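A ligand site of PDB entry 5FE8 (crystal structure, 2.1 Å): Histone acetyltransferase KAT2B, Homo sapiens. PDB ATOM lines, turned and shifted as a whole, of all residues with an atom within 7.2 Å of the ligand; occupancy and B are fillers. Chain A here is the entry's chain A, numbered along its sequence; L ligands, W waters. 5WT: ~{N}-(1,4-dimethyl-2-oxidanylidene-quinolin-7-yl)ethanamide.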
ATOM      1  N   TRP A  34     -23.543  -2.734  -7.148  1.00  0.00           N
ATOM      2  CA  TRP A  34     -22.737  -1.790  -6.371  1.00  0.00           C
ATOM      3  C   TRP A  34     -22.858  -0.279  -6.820  1.00  0.00           C
ATOM      4  O   TRP A  34     -22.792   0.608  -5.961  1.00  0.00           O
ATOM      5  CB  TRP A  34     -21.255  -2.234  -6.297  1.00  0.00           C
ATOM      6  CG  TRP A  34     -20.507  -2.198  -7.584  1.00  0.00           C
ATOM      7  CD1 TRP A  34     -20.294  -3.231  -8.436  1.00  0.00           C
ATOM      8  CD2 TRP A  34     -19.871  -1.044  -8.190  1.00  0.00           C
ATOM      9  NE1 TRP A  34     -19.567  -2.815  -9.539  1.00  0.00           N
ATOM     10  CE2 TRP A  34     -19.292  -1.488  -9.405  1.00  0.00           C
ATOM     11  CE3 TRP A  34     -19.719   0.288  -7.799  1.00  0.00           C
ATOM     12  CZ2 TRP A  34     -18.607  -0.632 -10.267  1.00  0.00           C
ATOM     13  CZ3 TRP A  34     -19.038   1.140  -8.641  1.00  0.00           C
ATOM     14  CH2 TRP A  34     -18.488   0.672  -9.878  1.00  0.00           C
ATOM     15  N   PRO A  35     -23.085  -0.004  -8.119  1.00  0.00           N
ATOM     16  CA  PRO A  35     -23.313   1.419  -8.533  1.00  0.00           C
ATOM     17  C   PRO A  35     -24.630   2.018  -8.056  1.00  0.00           C
ATOM     18  O   PRO A  35     -24.793   3.238  -8.092  1.00  0.00           O
ATOM     19  CB  PRO A  35     -23.359   1.337 -10.052  1.00  0.00           C
ATOM     20  CG  PRO A  35     -22.614   0.081 -10.385  1.00  0.00           C
ATOM     21  CD  PRO A  35     -23.099  -0.863  -9.325  1.00  0.00           C
ATOM     22  N   PHE A  36     -25.570   1.177  -7.627  1.00  0.00           N
ATOM     23  CA  PHE A  36     -26.979   1.555  -7.439  1.00  0.00           C
ATOM     24  C   PHE A  36     -27.458   1.436  -6.001  1.00  0.00           C
ATOM     25  O   PHE A  36     -28.654   1.670  -5.706  1.00  0.00           O
ATOM     26  CB  PHE A  36     -27.856   0.643  -8.308  1.00  0.00           C
ATOM     27  CG  PHE A  36     -27.355   0.528  -9.714  1.00  0.00           C
ATOM     28  CD1 PHE A  36     -27.304   1.662 -10.534  1.00  0.00           C
ATOM     29  CD2 PHE A  36     -26.878  -0.678 -10.215  1.00  0.00           C
ATOM     30  CE1 PHE A  36     -26.817   1.586 -11.832  1.00  0.00           C
ATOM     31  CE2 PHE A  36     -26.404  -0.772 -11.509  1.00  0.00           C
ATOM     32  CZ  PHE A  36     -26.391   0.378 -12.332  1.00  0.00           C
ATOM     33  N   MET A  37     -26.535   1.207  -5.074  1.00  0.00           N
ATOM     34  CA  MET A  37     -26.923   0.891  -3.676  1.00  0.00           C
ATOM     35  C   MET A  37     -27.424   2.118  -2.916  1.00  0.00           C
ATOM     36  O   MET A  37     -28.206   1.980  -1.978  1.00  0.00           O
ATOM     37  CB  MET A  37     -25.719   0.245  -2.897  1.00  0.00           C
ATOM     38  CG  MET A  37     -25.314  -1.095  -3.490  1.00  0.00           C
ATOM     39  SD  MET A  37     -26.584  -2.333  -3.265  1.00  0.00           S
ATOM     40  CE  MET A  37     -26.384  -2.628  -1.508  1.00  0.00           C
ATOM     41  N   GLU A  38     -26.940   3.307  -3.255  1.00  0.00           N
ATOM     42  CA  GLU A  38     -27.295   4.540  -2.528  1.00  0.00           C
ATOM     43  C   GLU A  38     -27.447   5.677  -3.522  1.00  0.00           C
ATOM     44  O   GLU A  38     -26.957   5.551  -4.642  1.00  0.00           O
ATOM     45  CB  GLU A  38     -26.166   4.897  -1.571  1.00  0.00           C
ATOM     46  CG  GLU A  38     -25.875   3.793  -0.595  1.00  0.00           C
ATOM     47  CD  GLU A  38     -25.181   4.291   0.635  1.00  0.00           C
ATOM     48  OE1 GLU A  38     -24.334   5.211   0.523  1.00  0.00           O
ATOM     49  OE2 GLU A  38     -25.535   3.751   1.705  1.00  0.00           O
ATOM     50  N   PRO A  39     -28.082   6.802  -3.120  1.00  0.00           N
ATOM     51  CA  PRO A  39     -28.155   7.931  -4.037  1.00  0.00           C
ATOM     52  C   PRO A  39     -26.807   8.294  -4.561  1.00  0.00           C
ATOM     53  O   PRO A  39     -25.850   8.395  -3.802  1.00  0.00           O
ATOM     54  CB  PRO A  39     -28.717   9.068  -3.183  1.00  0.00           C
ATOM     55  CG  PRO A  39     -29.498   8.382  -2.080  1.00  0.00           C
ATOM     56  CD  PRO A  39     -28.812   7.070  -1.854  1.00  0.00           C
ATOM     57  N   VAL A  40     -26.738   8.596  -5.827  1.00  0.00           N
ATOM     58  CA  VAL A  40     -25.484   9.094  -6.427  1.00  0.00           C
ATOM     59  C   VAL A  40     -24.990  10.335  -5.685  1.00  0.00           C
ATOM     60  O   VAL A  40     -25.756  11.249  -5.402  1.00  0.00           O
ATOM     61  CB  VAL A  40     -25.694   9.411  -7.922  1.00  0.00           C
ATOM     62  CG1 VAL A  40     -24.469  10.017  -8.548  1.00  0.00           C
ATOM     63  CG2 VAL A  40     -26.106   8.126  -8.677  1.00  0.00           C
ATOM     64  N   LYS A  41     -23.715  10.348  -5.326  1.00  0.00           N
ATOM     65  CA  LYS A  41     -23.141  11.494  -4.628  1.00  0.00           C
ATOM     66  C   LYS A  41     -22.623  12.535  -5.632  1.00  0.00           C
ATOM     67  O   LYS A  41     -21.978  12.177  -6.600  1.00  0.00           O
ATOM     68  CB  LYS A  41     -21.995  11.029  -3.723  1.00  0.00           C
ATOM     69  CG  LYS A  41     -22.441  10.177  -2.523  1.00  0.00           C
ATOM     70  CD  LYS A  41     -21.415   9.103  -2.184  1.00  0.00           C
ATOM     71  CE  LYS A  41     -21.809   8.257  -0.962  1.00  0.00           C
ATOM     72  NZ  LYS A  41     -22.841   7.228  -1.303  1.00  0.00           N
ATOM     73  N   GLU A  44     -19.144  12.138  -6.461  1.00  0.00           N
ATOM     74  CA  GLU A  44     -18.951  11.070  -7.468  1.00  0.00           C
ATOM     75  C   GLU A  44     -19.379  11.419  -8.887  1.00  0.00           C
ATOM     76  O   GLU A  44     -18.887  10.827  -9.858  1.00  0.00           O
ATOM     77  CB  GLU A  44     -19.735   9.789  -7.041  1.00  0.00           C
ATOM     78  CG  GLU A  44     -19.028   8.992  -5.944  1.00  0.00           C
ATOM     79  CD  GLU A  44     -19.919   7.989  -5.224  1.00  0.00           C
ATOM     80  OE1 GLU A  44     -21.111   7.819  -5.608  1.00  0.00           O
ATOM     81  OE2 GLU A  44     -19.394   7.355  -4.246  1.00  0.00           O
ATOM     82  N   ALA A  45     -20.349  12.317  -9.020  1.00  0.00           N
ATOM     83  CA  ALA A  45     -20.908  12.651 -10.333  1.00  0.00           C
ATOM     84  C   ALA A  45     -21.383  14.125 -10.319  1.00  0.00           C
ATOM     85  O   ALA A  45     -22.575  14.368 -10.208  1.00  0.00           O
ATOM     86  CB  ALA A  45     -22.027  11.709 -10.622  1.00  0.00           C
ATOM     87  N   PRO A  46     -20.449  15.103 -10.298  1.00  0.00           N
ATOM     88  CA  PRO A  46     -20.837  16.546 -10.232  1.00  0.00           C
ATOM     89  C   PRO A  46     -21.765  16.900 -11.406  1.00  0.00           C
ATOM     90  O   PRO A  46     -21.500  16.510 -12.550  1.00  0.00           O
ATOM     91  CB  PRO A  46     -19.503  17.278 -10.366  1.00  0.00           C
ATOM     92  CG  PRO A  46     -18.473  16.278  -9.991  1.00  0.00           C
ATOM     93  CD  PRO A  46     -18.995  14.953 -10.423  1.00  0.00           C
ATOM     94  N   TYR A  48     -24.780  15.623 -11.877  1.00  0.00           N
ATOM     95  CA  TYR A  48     -25.706  14.528 -12.064  1.00  0.00           C
ATOM     96  C   TYR A  48     -27.135  14.997 -11.832  1.00  0.00           C
ATOM     97  O   TYR A  48     -28.034  14.706 -12.617  1.00  0.00           O
ATOM     98  CB  TYR A  48     -25.383  13.384 -11.080  1.00  0.00           C
ATOM     99  CG  TYR A  48     -26.269  12.180 -11.228  1.00  0.00           C
ATOM    100  CD1 TYR A  48     -27.442  12.076 -10.516  1.00  0.00           C
ATOM    101  CD2 TYR A  48     -25.924  11.155 -12.083  1.00  0.00           C
ATOM    102  CE1 TYR A  48     -28.254  10.953 -10.644  1.00  0.00           C
ATOM    103  CE2 TYR A  48     -26.724  10.030 -12.230  1.00  0.00           C
ATOM    104  CZ  TYR A  48     -27.896   9.927 -11.528  1.00  0.00           C
ATOM    105  OH  TYR A  48     -28.668   8.775 -11.654  1.00  0.00           O
ATOM    106  N   ILE A  52     -30.408  14.423 -14.221  1.00  0.00           N
ATOM    107  CA  ILE A  52     -31.328  13.373 -13.869  1.00  0.00           C
ATOM    108  C   ILE A  52     -32.416  13.941 -12.928  1.00  0.00           C
ATOM    109  O   ILE A  52     -32.146  14.240 -11.779  1.00  0.00           O
ATOM    110  CB  ILE A  52     -30.543  12.187 -13.205  1.00  0.00           C
ATOM    111  CG1 ILE A  52     -29.542  11.583 -14.192  1.00  0.00           C
ATOM    112  CG2 ILE A  52     -31.476  11.116 -12.653  1.00  0.00           C
ATOM    113  CD1 ILE A  52     -30.180  11.058 -15.468  1.00  0.00           C
ATOM    114  N   MET A  56     -33.111   7.586  -8.501  1.00  0.00           N
ATOM    115  CA  MET A  56     -33.595   6.425  -7.752  1.00  0.00           C
ATOM    116  C   MET A  56     -32.413   5.499  -7.509  1.00  0.00           C
ATOM    117  O   MET A  56     -31.491   5.432  -8.304  1.00  0.00           O
ATOM    118  CB  MET A  56     -34.719   5.727  -8.483  1.00  0.00           C
ATOM    119  CG  MET A  56     -35.411   4.608  -7.705  1.00  0.00           C
ATOM    120  SD  MET A  56     -35.981   4.996  -6.041  1.00  0.00           S
ATOM    121  CE  MET A  56     -37.054   6.411  -6.293  1.00  0.00           C
ATOM    122  N   VAL A  83     -33.991   3.197 -11.949  1.00  0.00           N
ATOM    123  CA  VAL A  83     -32.583   3.050 -11.635  1.00  0.00           C
ATOM    124  C   VAL A  83     -31.809   2.789 -12.943  1.00  0.00           C
ATOM    125  O   VAL A  83     -30.721   3.388 -13.213  1.00  0.00           O
ATOM    126  CB  VAL A  83     -32.345   1.913 -10.604  1.00  0.00           C
ATOM    127  CG1 VAL A  83     -30.870   1.650 -10.403  1.00  0.00           C
ATOM    128  CG2 VAL A  83     -33.011   2.221  -9.255  1.00  0.00           C
ATOM    129  N   ASN A  86     -32.098   5.809 -15.635  1.00  0.00           N
ATOM    130  CA  ASN A  86     -31.194   6.939 -15.238  1.00  0.00           C
ATOM    131  C   ASN A  86     -29.750   6.643 -15.631  1.00  0.00           C
ATOM    132  O   ASN A  86     -29.068   7.479 -16.237  1.00  0.00           O
ATOM    133  CB  ASN A  86     -31.254   7.191 -13.759  1.00  0.00           C
ATOM    134  CG  ASN A  86     -32.546   7.837 -13.320  1.00  0.00           C
ATOM    135  OD1 ASN A  86     -33.286   8.364 -14.123  1.00  0.00           O
ATOM    136  ND2 ASN A  86     -32.761   7.840 -12.024  1.00  0.00           N
ATOM    137  N   CYS A  87     -29.293   5.434 -15.285  1.00  0.00           N
ATOM    138  CA  CYS A  87     -27.947   5.031 -15.604  1.00  0.00           C
ATOM    139  C   CYS A  87     -27.671   5.110 -17.122  1.00  0.00           C
ATOM    140  O   CYS A  87     -26.677   5.704 -17.588  1.00  0.00           O
ATOM    141  CB  CYS A  87     -27.700   3.645 -15.034  1.00  0.00           C
ATOM    142  SG  CYS A  87     -26.026   3.048 -15.315  1.00  0.00           S
ATOM    143  N   LYS A  88     -28.604   4.625 -17.909  1.00  0.00           N
ATOM    144  CA  LYS A  88     -28.413   4.614 -19.357  1.00  0.00           C
ATOM    145  C   LYS A  88     -28.566   6.002 -20.022  1.00  0.00           C
ATOM    146  O   LYS A  88     -27.915   6.261 -20.995  1.00  0.00           O
ATOM    147  CB  LYS A  88     -29.331   3.598 -19.984  1.00  0.00           C
ATOM    148  CG  LYS A  88     -29.039   2.178 -19.566  1.00  0.00           C
ATOM    149  CD  LYS A  88     -30.138   1.301 -20.016  1.00  0.00           C
ATOM    150  CE  LYS A  88     -29.883  -0.102 -19.603  1.00  0.00           C
ATOM    151  NZ  LYS A  88     -31.070  -0.933 -19.843  1.00  0.00           N
ATOM    152  N   TYR A  90     -27.542   8.739 -18.420  1.00  0.00           N
ATOM    153  CA  TYR A  90     -26.402   9.507 -17.932  1.00  0.00           C
ATOM    154  C   TYR A  90     -25.084   9.066 -18.534  1.00  0.00           C
ATOM    155  O   TYR A  90     -24.213   9.910 -18.779  1.00  0.00           O
ATOM    156  CB  TYR A  90     -26.319   9.455 -16.401  1.00  0.00           C
ATOM    157  CG  TYR A  90     -25.356  10.474 -15.847  1.00  0.00           C
ATOM    158  CD1 TYR A  90     -25.703  11.836 -15.820  1.00  0.00           C
ATOM    159  CD2 TYR A  90     -24.092  10.100 -15.388  1.00  0.00           C
ATOM    160  CE1 TYR A  90     -24.819  12.783 -15.296  1.00  0.00           C
ATOM    161  CE2 TYR A  90     -23.182  11.046 -14.880  1.00  0.00           C
ATOM    162  CZ  TYR A  90     -23.568  12.360 -14.818  1.00  0.00           C
ATOM    163  OH  TYR A  90     -22.723  13.303 -14.313  1.00  0.00           O
ATOM    164  N   ASN A  91     -24.914   7.759 -18.710  1.00  0.00           N
ATOM    165  CA  ASN A  91     -23.618   7.159 -19.025  1.00  0.00           C
ATOM    166  C   ASN A  91     -23.512   6.608 -20.449  1.00  0.00           C
ATOM    167  O   ASN A  91     -24.506   6.144 -20.974  1.00  0.00           O
ATOM    168  CB  ASN A  91     -23.343   6.017 -18.060  1.00  0.00           C
ATOM    169  CG  ASN A  91     -23.285   6.486 -16.640  1.00  0.00           C
ATOM    170  OD1 ASN A  91     -22.297   7.067 -16.218  1.00  0.00           O
ATOM    171  ND2 ASN A  91     -24.352   6.260 -15.879  1.00  0.00           N
ATOM    172  N   TYR A  97     -20.727   1.365 -15.553  1.00  0.00           N
ATOM    173  CA  TYR A  97     -22.053   1.596 -14.962  1.00  0.00           C
ATOM    174  C   TYR A  97     -23.182   1.078 -15.867  1.00  0.00           C
ATOM    175  O   TYR A  97     -24.063   0.385 -15.397  1.00  0.00           O
ATOM    176  CB  TYR A  97     -22.306   3.069 -14.635  1.00  0.00           C
ATOM    177  CG  TYR A  97     -21.296   3.678 -13.736  1.00  0.00           C
ATOM    178  CD1 TYR A  97     -21.000   3.144 -12.473  1.00  0.00           C
ATOM    179  CD2 TYR A  97     -20.577   4.774 -14.161  1.00  0.00           C
ATOM    180  CE1 TYR A  97     -20.034   3.740 -11.668  1.00  0.00           C
ATOM    181  CE2 TYR A  97     -19.631   5.356 -13.384  1.00  0.00           C
ATOM    182  CZ  TYR A  97     -19.346   4.840 -12.150  1.00  0.00           C
ATOM    183  OH  TYR A  97     -18.382   5.492 -11.429  1.00  0.00           O
ATOM    184  N   TYR A  98     -23.104   1.390 -17.181  1.00  0.00           N
ATOM    185  CA  TYR A  98     -24.111   0.945 -18.152  1.00  0.00           C
ATOM    186  C   TYR A  98     -24.092  -0.586 -18.215  1.00  0.00           C
ATOM    187  O   TYR A  98     -25.127  -1.212 -18.136  1.00  0.00           O
ATOM    188  CB  TYR A  98     -23.877   1.604 -19.535  1.00  0.00           C
ATOM    189  CG  TYR A  98     -25.048   1.502 -20.544  1.00  0.00           C
ATOM    190  CD1 TYR A  98     -25.500   0.267 -21.017  1.00  0.00           C
ATOM    191  CD2 TYR A  98     -25.633   2.663 -21.080  1.00  0.00           C
ATOM    192  CE1 TYR A  98     -26.528   0.174 -21.986  1.00  0.00           C
ATOM    193  CE2 TYR A  98     -26.685   2.590 -22.018  1.00  0.00           C
ATOM    194  CZ  TYR A  98     -27.131   1.348 -22.481  1.00  0.00           C
ATOM    195  OH  TYR A  98     -28.171   1.190 -23.424  1.00  0.00           O
HETATM  196  CAB 5WT L   1     -20.784   8.671 -12.548  1.00  0.00           C
HETATM  197  CAM 5WT L   1     -21.816   7.795 -12.081  1.00  0.00           C
HETATM  198  CAH 5WT L   1     -22.926   7.540 -12.890  1.00  0.00           C
HETATM  199  CAN 5WT L   1     -23.966   6.665 -12.487  1.00  0.00           C
HETATM  200  OAE 5WT L   1     -24.937   6.480 -13.234  1.00  0.00           O
HETATM  201  NAQ 5WT L   1     -23.887   6.039 -11.316  1.00  0.00           N
HETATM  202  CAC 5WT L   1     -25.047   5.151 -10.991  1.00  0.00           C
HETATM  203  CAP 5WT L   1     -22.804   6.262 -10.467  1.00  0.00           C
HETATM  204  CAI 5WT L   1     -22.689   5.622  -9.218  1.00  0.00           C
HETATM  205  CAO 5WT L   1     -21.730   7.132 -10.854  1.00  0.00           C
HETATM  206  CAG 5WT L   1     -20.626   7.334  -9.994  1.00  0.00           C
HETATM  207  CAF 5WT L   1     -20.572   6.696  -8.768  1.00  0.00           C
HETATM  208  CAL 5WT L   1     -21.602   5.817  -8.374  1.00  0.00           C
HETATM  209  NAJ 5WT L   1     -21.658   5.163  -7.203  1.00  0.00           N
HETATM  210  CAK 5WT L   1     -20.571   4.612  -6.637  1.00  0.00           C
HETATM  211  OAD 5WT L   1     -19.417   4.642  -7.087  1.00  0.00           O
HETATM  212  CAA 5WT L   1     -20.873   3.912  -5.286  1.00  0.00           C
HETATM  213  O   HOH W   1     -27.672   6.812 -12.893  1.00  0.00           O
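ND2 of Asn 91 sits at hydrogen-bond distance from OAE of the ligand (2.7 Å).
The side-chain carboxylate (OE1) of Glu 44 sits at hydrogen-bond distance from a nitrogen (NAJ) of the ligand (3.1 Å).
The side-chain amide nitrogen of Asn 91 sits at hydrogen-bond distance from the backbone carbonyl oxygen of Cys 87, at 2.9 Å.
The backbone carbonyl oxygen (O) of Tyr 97 is in hydrogen-bond range of the side-chain sulfur (SG) of Cys 87, at 3.3 Å.
CZ3 of Trp 34 touches OAD of the ligand (3.9 Å).
O of Pro 35 touches CAI of the ligand, at 3.4 Å.
Val 40 touches the ligand.
CB of Ala 45 touches CAB of the ligand (3.8 Å).
CD2 of Tyr 90 touches CAH of the ligand, 3.8 Å away.
Tyr 97 touches the ligand.
Hydrophobic or aromatic side chains that line the ligand: Trp 34, Val 40, Ala 45, Tyr 90 and Tyr 97.
Eight residues have an atom within 4 Å of the ligand: Trp 34, Pro 35, Val 40, Glu 44, Ala 45, Tyr 90, Asn 91 and Tyr 97.
Water W1 lies within hydrogen-bond range of the side-chain hydroxyl of Tyr 48 (2.5 Å), an oxygen (OAE) of the ligand (2.8 Å) and the backbone NH of Cys 87 (3.2 Å).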
